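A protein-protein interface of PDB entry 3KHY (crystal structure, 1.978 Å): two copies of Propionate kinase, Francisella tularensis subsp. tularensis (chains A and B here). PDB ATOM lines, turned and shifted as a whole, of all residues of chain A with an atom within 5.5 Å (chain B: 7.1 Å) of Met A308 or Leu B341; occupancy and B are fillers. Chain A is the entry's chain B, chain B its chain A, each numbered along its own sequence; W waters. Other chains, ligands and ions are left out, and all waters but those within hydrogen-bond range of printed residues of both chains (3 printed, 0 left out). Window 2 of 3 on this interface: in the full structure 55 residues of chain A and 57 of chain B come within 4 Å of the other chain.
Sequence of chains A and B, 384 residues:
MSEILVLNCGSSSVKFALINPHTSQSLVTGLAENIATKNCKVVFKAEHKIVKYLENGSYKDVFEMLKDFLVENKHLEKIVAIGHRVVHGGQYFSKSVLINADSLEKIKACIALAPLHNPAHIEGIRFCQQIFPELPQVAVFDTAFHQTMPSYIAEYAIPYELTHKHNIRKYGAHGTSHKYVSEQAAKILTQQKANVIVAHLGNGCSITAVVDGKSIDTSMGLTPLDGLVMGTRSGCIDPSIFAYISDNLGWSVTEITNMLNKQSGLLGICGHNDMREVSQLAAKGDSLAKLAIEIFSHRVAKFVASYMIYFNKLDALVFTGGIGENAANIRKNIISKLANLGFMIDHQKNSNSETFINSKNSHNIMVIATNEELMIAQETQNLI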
ATOM      1  N   ILE A 197     -11.815 -12.849 -18.276  1.00  0.00           N
ATOM      2  CA  ILE A 197     -10.774 -13.579 -18.977  1.00  0.00           C
ATOM      3  C   ILE A 197     -10.453 -12.763 -20.224  1.00  0.00           C
ATOM      4  O   ILE A 197     -11.356 -12.416 -20.982  1.00  0.00           O
ATOM      5  CB  ILE A 197     -11.255 -14.989 -19.356  1.00  0.00           C
ATOM      6  CG1 ILE A 197     -11.568 -15.795 -18.086  1.00  0.00           C
ATOM      7  CG2 ILE A 197     -10.218 -15.699 -20.227  1.00  0.00           C
ATOM      8  CD1 ILE A 197     -12.323 -17.095 -18.335  1.00  0.00           C
ATOM      9  N   PHE A 303      -8.149 -23.074 -22.950  1.00  0.00           N
ATOM     10  CA  PHE A 303      -7.664 -22.196 -21.893  1.00  0.00           C
ATOM     11  C   PHE A 303      -8.807 -21.418 -21.224  1.00  0.00           C
ATOM     12  O   PHE A 303      -8.834 -21.262 -20.002  1.00  0.00           O
ATOM     13  CB  PHE A 303      -6.598 -21.233 -22.439  1.00  0.00           C
ATOM     14  CG  PHE A 303      -5.182 -21.773 -22.319  1.00  0.00           C
ATOM     15  CD1 PHE A 303      -4.369 -21.405 -21.253  1.00  0.00           C
ATOM     16  CD2 PHE A 303      -4.693 -22.669 -23.250  1.00  0.00           C
ATOM     17  CE1 PHE A 303      -3.076 -21.910 -21.129  1.00  0.00           C
ATOM     18  CE2 PHE A 303      -3.393 -23.181 -23.140  1.00  0.00           C
ATOM     19  CZ  PHE A 303      -2.583 -22.783 -22.079  1.00  0.00           C
ATOM     20  N   VAL A 304      -9.745 -20.935 -22.024  1.00  0.00           N
ATOM     21  CA  VAL A 304     -10.878 -20.198 -21.478  1.00  0.00           C
ATOM     22  C   VAL A 304     -11.638 -21.122 -20.526  1.00  0.00           C
ATOM     23  O   VAL A 304     -12.008 -20.734 -19.409  1.00  0.00           O
ATOM     24  CB  VAL A 304     -11.832 -19.722 -22.577  1.00  0.00           C
ATOM     25  CG1 VAL A 304     -13.118 -19.199 -21.944  1.00  0.00           C
ATOM     26  CG2 VAL A 304     -11.167 -18.630 -23.465  1.00  0.00           C
ATOM     27  N   ALA A 305     -11.874 -22.348 -20.980  1.00  0.00           N
ATOM     28  CA  ALA A 305     -12.547 -23.340 -20.154  1.00  0.00           C
ATOM     29  C   ALA A 305     -11.827 -23.578 -18.849  1.00  0.00           C
ATOM     30  O   ALA A 305     -12.453 -23.648 -17.797  1.00  0.00           O
ATOM     31  CB  ALA A 305     -12.696 -24.661 -20.908  1.00  0.00           C
ATOM     32  N   SER A 306     -10.505 -23.715 -18.909  1.00  0.00           N
ATOM     33  CA  SER A 306      -9.731 -24.000 -17.708  1.00  0.00           C
ATOM     34  C   SER A 306      -9.783 -22.845 -16.718  1.00  0.00           C
ATOM     35  O   SER A 306      -9.779 -23.071 -15.507  1.00  0.00           O
ATOM     36  CB  SER A 306      -8.270 -24.333 -18.043  1.00  0.00           C
ATOM     37  OG  SER A 306      -7.519 -23.165 -18.327  1.00  0.00           O
ATOM     38  N   TYR A 307      -9.817 -21.614 -17.226  1.00  0.00           N
ATOM     39  CA  TYR A 307      -9.823 -20.442 -16.355  1.00  0.00           C
ATOM     40  C   TYR A 307     -11.185 -20.171 -15.727  1.00  0.00           C
ATOM     41  O   TYR A 307     -11.286 -19.340 -14.845  1.00  0.00           O
ATOM     42  CB  TYR A 307      -9.338 -19.185 -17.077  1.00  0.00           C
ATOM     43  CG  TYR A 307      -7.857 -19.169 -17.427  1.00  0.00           C
ATOM     44  CD1 TYR A 307      -7.003 -20.188 -17.010  1.00  0.00           C
ATOM     45  CD2 TYR A 307      -7.324 -18.138 -18.203  1.00  0.00           C
ATOM     46  CE1 TYR A 307      -5.650 -20.179 -17.350  1.00  0.00           C
ATOM     47  CE2 TYR A 307      -5.978 -18.117 -18.536  1.00  0.00           C
ATOM     48  CZ  TYR A 307      -5.150 -19.131 -18.111  1.00  0.00           C
ATOM     49  OH  TYR A 307      -3.816 -19.099 -18.452  1.00  0.00           O
ATOM     50  N   MET A 308     -12.225 -20.873 -16.167  1.00  0.00           N
ATOM     51  CA  MET A 308     -13.536 -20.753 -15.517  1.00  0.00           C
ATOM     52  C   MET A 308     -13.471 -21.134 -14.038  1.00  0.00           C
ATOM     53  O   MET A 308     -14.310 -20.718 -13.240  1.00  0.00           O
ATOM     54  CB  MET A 308     -14.599 -21.601 -16.242  1.00  0.00           C
ATOM     55  CG  MET A 308     -14.826 -21.177 -17.688  1.00  0.00           C
ATOM     56  SD  MET A 308     -15.490 -19.357 -17.854  1.00  0.00           S
ATOM     57  CE  MET A 308     -17.342 -19.603 -17.275  1.00  0.00           C
ATOM     58  N   ILE A 309     -12.450 -21.901 -13.687  1.00  0.00           N
ATOM     59  CA  ILE A 309     -12.267 -22.372 -12.328  1.00  0.00           C
ATOM     60  C   ILE A 309     -12.153 -21.216 -11.327  1.00  0.00           C
ATOM     61  O   ILE A 309     -12.478 -21.370 -10.149  1.00  0.00           O
ATOM     62  CB  ILE A 309     -11.002 -23.245 -12.248  1.00  0.00           C
ATOM     63  CG1 ILE A 309     -10.998 -24.092 -10.982  1.00  0.00           C
ATOM     64  CG2 ILE A 309      -9.747 -22.382 -12.343  1.00  0.00           C
ATOM     65  CD1 ILE A 309      -9.801 -25.005 -10.894  1.00  0.00           C
ATOM     66  N   TYR A 310     -11.702 -20.058 -11.806  1.00  0.00           N
ATOM     67  CA  TYR A 310     -11.423 -18.917 -10.934  1.00  0.00           C
ATOM     68  C   TYR A 310     -12.624 -18.028 -10.606  1.00  0.00           C
ATOM     69  O   TYR A 310     -12.504 -17.126  -9.775  1.00  0.00           O
ATOM     70  CB  TYR A 310     -10.323 -18.044 -11.537  1.00  0.00           C
ATOM     71  CG  TYR A 310      -9.021 -18.790 -11.728  1.00  0.00           C
ATOM     72  CD1 TYR A 310      -8.290 -19.237 -10.628  1.00  0.00           C
ATOM     73  CD2 TYR A 310      -8.525 -19.035 -12.993  1.00  0.00           C
ATOM     74  CE1 TYR A 310      -7.107 -19.923 -10.784  1.00  0.00           C
ATOM     75  CE2 TYR A 310      -7.317 -19.734 -13.169  1.00  0.00           C
ATOM     76  CZ  TYR A 310      -6.618 -20.160 -12.057  1.00  0.00           C
ATOM     77  OH  TYR A 310      -5.428 -20.843 -12.209  1.00  0.00           O
ATOM     78  N   PHE A 311     -13.765 -18.276 -11.238  1.00  0.00           N
ATOM     79  CA  PHE A 311     -14.872 -17.328 -11.181  1.00  0.00           C
ATOM     80  C   PHE A 311     -16.171 -17.865 -10.576  1.00  0.00           C
ATOM     81  O   PHE A 311     -16.784 -18.781 -11.106  1.00  0.00           O
ATOM     82  CB  PHE A 311     -15.146 -16.761 -12.583  1.00  0.00           C
ATOM     83  CG  PHE A 311     -13.962 -16.042 -13.179  1.00  0.00           C
ATOM     84  CD1 PHE A 311     -13.687 -14.724 -12.825  1.00  0.00           C
ATOM     85  CD2 PHE A 311     -13.111 -16.694 -14.070  1.00  0.00           C
ATOM     86  CE1 PHE A 311     -12.590 -14.054 -13.369  1.00  0.00           C
ATOM     87  CE2 PHE A 311     -12.015 -16.048 -14.602  1.00  0.00           C
ATOM     88  CZ  PHE A 311     -11.748 -14.726 -14.259  1.00  0.00           C
ATOM     89  N   LEU A 314     -18.371 -14.856 -13.784  1.00  0.00           N
ATOM     90  CA  LEU A 314     -17.511 -14.257 -14.797  1.00  0.00           C
ATOM     91  C   LEU A 314     -18.169 -12.998 -15.352  1.00  0.00           C
ATOM     92  O   LEU A 314     -19.280 -13.071 -15.864  1.00  0.00           O
ATOM     93  CB  LEU A 314     -17.275 -15.252 -15.940  1.00  0.00           C
ATOM     94  CG  LEU A 314     -16.431 -14.729 -17.113  1.00  0.00           C
ATOM     95  CD1 LEU A 314     -15.016 -14.438 -16.654  1.00  0.00           C
ATOM     96  CD2 LEU A 314     -16.412 -15.724 -18.300  1.00  0.00           C
ATOM     97  N   LEU A 341     -20.127 -24.414 -22.469  1.00  0.00           N
ATOM     98  CA  LEU A 341     -19.868 -23.635 -21.263  1.00  0.00           C
ATOM     99  C   LEU A 341     -20.756 -22.392 -21.174  1.00  0.00           C
ATOM    100  O   LEU A 341     -20.530 -21.527 -20.336  1.00  0.00           O
ATOM    101  CB  LEU A 341     -18.396 -23.234 -21.193  1.00  0.00           C
ATOM    102  CG  LEU A 341     -17.440 -24.234 -20.524  1.00  0.00           C
ATOM    103  CD1 LEU A 341     -17.532 -25.592 -21.176  1.00  0.00           C
ATOM    104  CD2 LEU A 341     -16.016 -23.727 -20.570  1.00  0.00           C
ATOM    105  N   PHE A 343     -21.400 -20.064 -23.626  1.00  0.00           N
ATOM    106  CA  PHE A 343     -21.024 -18.922 -24.448  1.00  0.00           C
ATOM    107  C   PHE A 343     -21.768 -19.049 -25.769  1.00  0.00           C
ATOM    108  O   PHE A 343     -21.872 -20.145 -26.320  1.00  0.00           O
ATOM    109  CB  PHE A 343     -19.512 -18.893 -24.703  1.00  0.00           C
ATOM    110  CG  PHE A 343     -18.677 -18.593 -23.471  1.00  0.00           C
ATOM    111  CD1 PHE A 343     -18.251 -19.618 -22.642  1.00  0.00           C
ATOM    112  CD2 PHE A 343     -18.301 -17.293 -23.169  1.00  0.00           C
ATOM    113  CE1 PHE A 343     -17.479 -19.360 -21.520  1.00  0.00           C
ATOM    114  CE2 PHE A 343     -17.526 -17.016 -22.037  1.00  0.00           C
ATOM    115  CZ  PHE A 343     -17.117 -18.057 -21.215  1.00  0.00           C
ATOM    116  N   HIS A 363     -22.741 -15.713 -21.410  1.00  0.00           N
ATOM    117  CA  HIS A 363     -21.862 -14.837 -20.657  1.00  0.00           C
ATOM    118  C   HIS A 363     -21.571 -13.662 -21.575  1.00  0.00           C
ATOM    119  O   HIS A 363     -21.635 -13.811 -22.796  1.00  0.00           O
ATOM    120  CB  HIS A 363     -20.536 -15.539 -20.338  1.00  0.00           C
ATOM    121  CG  HIS A 363     -20.681 -16.784 -19.521  1.00  0.00           C
ATOM    122  ND1 HIS A 363     -20.995 -16.762 -18.180  1.00  0.00           N
ATOM    123  CD2 HIS A 363     -20.536 -18.089 -19.852  1.00  0.00           C
ATOM    124  CE1 HIS A 363     -21.052 -18.001 -17.721  1.00  0.00           C
ATOM    125  NE2 HIS A 363     -20.779 -18.825 -18.718  1.00  0.00           N
ATOM    126  N   ALA B 301      -7.401 -29.928 -11.189  1.00  0.00           N
ATOM    127  CA  ALA B 301      -8.617 -29.133 -11.329  1.00  0.00           C
ATOM    128  C   ALA B 301      -8.632 -28.319 -12.624  1.00  0.00           C
ATOM    129  O   ALA B 301      -9.669 -28.229 -13.277  1.00  0.00           O
ATOM    130  CB  ALA B 301      -8.821 -28.225 -10.119  1.00  0.00           C
ATOM    131  N   LYS B 302      -7.492 -27.730 -13.006  1.00  0.00           N
ATOM    132  CA  LYS B 302      -7.416 -26.991 -14.265  1.00  0.00           C
ATOM    133  C   LYS B 302      -7.705 -27.854 -15.508  1.00  0.00           C
ATOM    134  O   LYS B 302      -8.372 -27.393 -16.442  1.00  0.00           O
ATOM    135  CB  LYS B 302      -6.066 -26.265 -14.414  1.00  0.00           C
ATOM    136  CG  LYS B 302      -6.051 -24.922 -13.688  1.00  0.00           C
ATOM    137  CD  LYS B 302      -4.719 -24.224 -13.787  1.00  0.00           C
ATOM    138  CE  LYS B 302      -4.443 -23.749 -15.204  1.00  0.00           C
ATOM    139  NZ  LYS B 302      -3.129 -23.059 -15.229  1.00  0.00           N
ATOM    140  N   VAL B 304      -9.495 -30.738 -15.474  1.00  0.00           N
ATOM    141  CA  VAL B 304     -10.904 -31.067 -15.397  1.00  0.00           C
ATOM    142  C   VAL B 304     -11.719 -29.932 -15.993  1.00  0.00           C
ATOM    143  O   VAL B 304     -12.566 -30.151 -16.854  1.00  0.00           O
ATOM    144  CB  VAL B 304     -11.359 -31.267 -13.946  1.00  0.00           C
ATOM    145  CG1 VAL B 304     -12.882 -31.381 -13.892  1.00  0.00           C
ATOM    146  CG2 VAL B 304     -10.693 -32.510 -13.353  1.00  0.00           C
ATOM    147  N   ALA B 305     -11.460 -28.714 -15.528  1.00  0.00           N
ATOM    148  CA  ALA B 305     -12.169 -27.538 -16.044  1.00  0.00           C
ATOM    149  C   ALA B 305     -12.029 -27.400 -17.558  1.00  0.00           C
ATOM    150  O   ALA B 305     -13.011 -27.101 -18.268  1.00  0.00           O
ATOM    151  CB  ALA B 305     -11.680 -26.266 -15.349  1.00  0.00           C
ATOM    152  N   SER B 306     -10.817 -27.624 -18.067  1.00  0.00           N
ATOM    153  CA  SER B 306     -10.562 -27.455 -19.498  1.00  0.00           C
ATOM    154  C   SER B 306     -11.316 -28.495 -20.312  1.00  0.00           C
ATOM    155  O   SER B 306     -11.727 -28.229 -21.441  1.00  0.00           O
ATOM    156  CB  SER B 306      -9.062 -27.525 -19.822  1.00  0.00           C
ATOM    157  OG  SER B 306      -8.638 -28.854 -20.064  1.00  0.00           O
ATOM    158  N   MET B 308     -14.262 -29.694 -19.595  1.00  0.00           N
ATOM    159  CA  MET B 308     -15.703 -29.449 -19.591  1.00  0.00           C
ATOM    160  C   MET B 308     -16.219 -29.041 -20.983  1.00  0.00           C
ATOM    161  O   MET B 308     -17.387 -29.259 -21.297  1.00  0.00           O
ATOM    162  CB  MET B 308     -16.076 -28.386 -18.552  1.00  0.00           C
ATOM    163  CG  MET B 308     -15.736 -28.780 -17.122  1.00  0.00           C
ATOM    164  SD  MET B 308     -16.665 -30.439 -16.577  1.00  0.00           S
ATOM    165  CE  MET B 308     -18.437 -29.659 -16.238  1.00  0.00           C
ATOM    166  N   LYS B 337     -11.248 -27.187  -5.242  1.00  0.00           N
ATOM    167  CA  LYS B 337     -10.813 -26.216  -6.243  1.00  0.00           C
ATOM    168  C   LYS B 337     -11.770 -26.125  -7.432  1.00  0.00           C
ATOM    169  O   LYS B 337     -11.659 -25.226  -8.256  1.00  0.00           O
ATOM    170  CB  LYS B 337      -9.377 -26.527  -6.687  1.00  0.00           C
ATOM    171  CG  LYS B 337      -8.365 -26.194  -5.579  1.00  0.00           C
ATOM    172  CD  LYS B 337      -6.947 -26.623  -5.904  1.00  0.00           C
ATOM    173  CE  LYS B 337      -5.948 -25.964  -4.938  1.00  0.00           C
ATOM    174  NZ  LYS B 337      -6.278 -26.179  -3.487  1.00  0.00           N
ATOM    175  N   LEU B 338     -12.702 -27.072  -7.517  1.00  0.00           N
ATOM    176  CA  LEU B 338     -13.674 -27.117  -8.604  1.00  0.00           C
ATOM    177  C   LEU B 338     -15.046 -26.582  -8.161  1.00  0.00           C
ATOM    178  O   LEU B 338     -16.040 -26.754  -8.853  1.00  0.00           O
ATOM    179  CB  LEU B 338     -13.820 -28.544  -9.134  1.00  0.00           C
ATOM    180  CG  LEU B 338     -12.619 -29.019  -9.967  1.00  0.00           C
ATOM    181  CD1 LEU B 338     -12.599 -30.547 -10.090  1.00  0.00           C
ATOM    182  CD2 LEU B 338     -12.584 -28.360 -11.344  1.00  0.00           C
ATOM    183  N   ALA B 339     -15.078 -25.904  -7.023  1.00  0.00           N
ATOM    184  CA  ALA B 339     -16.331 -25.382  -6.478  1.00  0.00           C
ATOM    185  C   ALA B 339     -17.105 -24.515  -7.482  1.00  0.00           C
ATOM    186  O   ALA B 339     -18.320 -24.635  -7.595  1.00  0.00           O
ATOM    187  CB  ALA B 339     -16.072 -24.609  -5.183  1.00  0.00           C
ATOM    188  N   ASN B 340     -16.411 -23.649  -8.216  1.00  0.00           N
ATOM    189  CA  ASN B 340     -17.109 -22.733  -9.125  1.00  0.00           C
ATOM    190  C   ASN B 340     -17.696 -23.426 -10.349  1.00  0.00           C
ATOM    191  O   ASN B 340     -18.448 -22.816 -11.119  1.00  0.00           O
ATOM    192  CB  ASN B 340     -16.205 -21.573  -9.557  1.00  0.00           C
ATOM    193  CG  ASN B 340     -15.821 -20.676  -8.398  1.00  0.00           C
ATOM    194  OD1 ASN B 340     -16.643 -20.391  -7.523  1.00  0.00           O
ATOM    195  ND2 ASN B 340     -14.571 -20.210  -8.394  1.00  0.00           N
ATOM    196  N   LEU B 341     -17.359 -24.701 -10.529  1.00  0.00           N
ATOM    197  CA  LEU B 341     -17.869 -25.461 -11.663  1.00  0.00           C
ATOM    198  C   LEU B 341     -18.967 -26.455 -11.277  1.00  0.00           C
ATOM    199  O   LEU B 341     -19.293 -27.348 -12.058  1.00  0.00           O
ATOM    200  CB  LEU B 341     -16.735 -26.223 -12.354  1.00  0.00           C
ATOM    201  CG  LEU B 341     -15.895 -25.494 -13.405  1.00  0.00           C
ATOM    202  CD1 LEU B 341     -15.237 -24.278 -12.810  1.00  0.00           C
ATOM    203  CD2 LEU B 341     -14.850 -26.436 -13.988  1.00  0.00           C
ATOM    204  N   GLY B 342     -19.526 -26.317 -10.082  1.00  0.00           N
ATOM    205  CA  GLY B 342     -20.637 -27.169  -9.690  1.00  0.00           C
ATOM    206  C   GLY B 342     -20.251 -28.566  -9.218  1.00  0.00           C
ATOM    207  O   GLY B 342     -21.024 -29.506  -9.393  1.00  0.00           O
ATOM    208  N   PHE B 343     -19.058 -28.704  -8.634  1.00  0.00           N
ATOM    209  CA  PHE B 343     -18.635 -29.942  -7.977  1.00  0.00           C
ATOM    210  C   PHE B 343     -18.623 -29.738  -6.470  1.00  0.00           C
ATOM    211  O   PHE B 343     -18.108 -28.732  -5.974  1.00  0.00           O
ATOM    212  CB  PHE B 343     -17.217 -30.361  -8.419  1.00  0.00           C
ATOM    213  CG  PHE B 343     -17.112 -30.740  -9.878  1.00  0.00           C
ATOM    214  CD1 PHE B 343     -16.856 -29.778 -10.842  1.00  0.00           C
ATOM    215  CD2 PHE B 343     -17.259 -32.062 -10.277  1.00  0.00           C
ATOM    216  CE1 PHE B 343     -16.753 -30.120 -12.191  1.00  0.00           C
ATOM    217  CE2 PHE B 343     -17.171 -32.413 -11.621  1.00  0.00           C
ATOM    218  CZ  PHE B 343     -16.911 -31.441 -12.578  1.00  0.00           C
ATOM    219  N   MET B 344     -19.171 -30.703  -5.738  1.00  0.00           N
ATOM    220  CA  MET B 344     -19.191 -30.640  -4.274  1.00  0.00           C
ATOM    221  C   MET B 344     -19.083 -32.040  -3.730  1.00  0.00           C
ATOM    222  O   MET B 344     -19.817 -32.931  -4.162  1.00  0.00           O
ATOM    223  CB  MET B 344     -20.500 -30.036  -3.767  1.00  0.00           C
ATOM    224  CG  MET B 344     -20.772 -28.631  -4.290  1.00  0.00           C
ATOM    225  SD  MET B 344     -19.622 -27.325  -3.399  1.00  0.00           S
ATOM    226  CE  MET B 344     -19.864 -27.927  -1.552  1.00  0.00           C
ATOM    227  N   SER B 362     -24.371 -31.285  -7.165  1.00  0.00           N
ATOM    228  CA  SER B 362     -23.051 -31.502  -7.737  1.00  0.00           C
ATOM    229  C   SER B 362     -23.137 -32.404  -8.938  1.00  0.00           C
ATOM    230  O   SER B 362     -24.014 -33.258  -9.012  1.00  0.00           O
ATOM    231  CB  SER B 362     -22.130 -32.159  -6.696  1.00  0.00           C
ATOM    232  OG  SER B 362     -20.854 -32.457  -7.261  1.00  0.00           O
ATOM    233  N   HIS B 363     -22.229 -32.205  -9.885  1.00  0.00           N
ATOM    234  CA  HIS B 363     -21.916 -33.240 -10.857  1.00  0.00           C
ATOM    235  C   HIS B 363     -21.568 -34.507 -10.099  1.00  0.00           C
ATOM    236  O   HIS B 363     -21.076 -34.445  -8.971  1.00  0.00           O
ATOM    237  CB  HIS B 363     -20.699 -32.843 -11.686  1.00  0.00           C
ATOM    238  CG  HIS B 363     -20.912 -31.624 -12.533  1.00  0.00           C
ATOM    239  ND1 HIS B 363     -21.875 -31.560 -13.515  1.00  0.00           N
ATOM    240  CD2 HIS B 363     -20.284 -30.425 -12.541  1.00  0.00           C
ATOM    241  CE1 HIS B 363     -21.825 -30.375 -14.100  1.00  0.00           C
ATOM    242  NE2 HIS B 363     -20.871 -29.667 -13.521  1.00  0.00           N
HETATM  243  O   HOH W   1     -14.757 -25.122 -17.522  1.00  0.00           O
HETATM  244  O   HOH W   2      -2.602 -21.277 -17.419  1.00  0.00           O
HETATM  245  O   HOH W   3     -13.603 -23.559  -8.843  1.00  0.00           O
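Of the printed residues of chain B, Ala A305 touches Ala B305 and Ser B306. Tyr A307 touches none of the printed residues of chain B. Met A308 touches just one residue of chain B: Leu B341. Printed residues of chain A within 4 Å of Ala B301: Ile A309. Of the printed residues of chain A, Lys B302 touches Ser A306 (3.5 Å) and Tyr A310 (3.8 Å). Of the printed residues of chain A, Ala B305 touches Ala A305 and Ser A306. Printed residues of chain A within 4 Å of Met B308: Leu A341 (3.7 Å). Of the printed residues of chain A, Leu B341 touches Met A308 (3.7 Å) and Ile A309 (3.6 Å). Phe B343 touches none of the printed residues of chain A. The nearest printed residue of chain A that does not touch Leu B341 is Ala A305 (5.3 Å). The nearest printed residue of chain B that does not touch Leu A341 is Ala B305 (5.1 Å).
Hydrophobic or aromatic side chains of chain B within 4 Å of the printed part of chain A: Ala B301, Ala B305 and Leu B341. Of the 14 printed residues of chain A, 7 touch a printed residue of chain B. Printed residues of chain A that touch a printed residue of chain B: Ala A305, Ser A306, Met A308, Ile A309, Tyr A310, Phe A311 and Leu A341. Among the printed residues, 14 pairs touch across the chains.
Water W3 lies within hydrogen-bond range of O of Lys B337, O of Ile A309, N of Asn B340 and N of Ala B339. Water W2 bridges OH of Tyr A307 and NZ of Lys B302. Water W1 bridges O of Ala B305 (2.7 Å) and O of Ala A305 (2.7 Å).
The backbone carbonyl oxygen of Ile A309 lies within hydrogen-bond range of the side-chain amide nitrogen of Asn B340, at 3.0 Å.
Ala B305 touches Ala A305 (O to O, 3.5 Å). Ser B306 touches Ala A305 (O to CB, 3.7 Å). Ser A306 touches Lys B302. O of Ser A306 touches CB of Ala B305 (3.7 Å). Ile A309 touches Ala B301. Lys B337 touches Ile A309. CA of Ile A309 touches CD1 of Leu B341, at 3.6 Å. Tyr A310 touches Lys B302. C of Tyr A310 touches ND2 of Asn B340 (3.7 Å). O of Phe A311 touches CB of Asn B340, at 3.2 Å.
The backbone carbonyl oxygen (O) of Leu B341 lies within hydrogen-bond range of a ring nitrogen (NE2) of His B363. The backbone carbonyl oxygen (O) of Phe A303 lies within hydrogen-bond range of the side-chain hydroxyl (OG) of Ser A306 (2.9 Å). A ring nitrogen (NE2) of His A363 lies within hydrogen-bond range of the backbone carbonyl oxygen (O) of Leu A341.
Ala B305 touches its own counterpart, Ala A305. Ala A305 touches Ser B306, and with the chains exchanged Ser A306 touches Ala B305. Ser B306 touches its own counterpart, Ser A306. Met A308 touches Leu B341, and with the chains exchanged Leu A341 touches Met B308. Of the 14 pairs that touch across the chains among the printed residues, 6 have their exchanged pair printed and touching as well.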
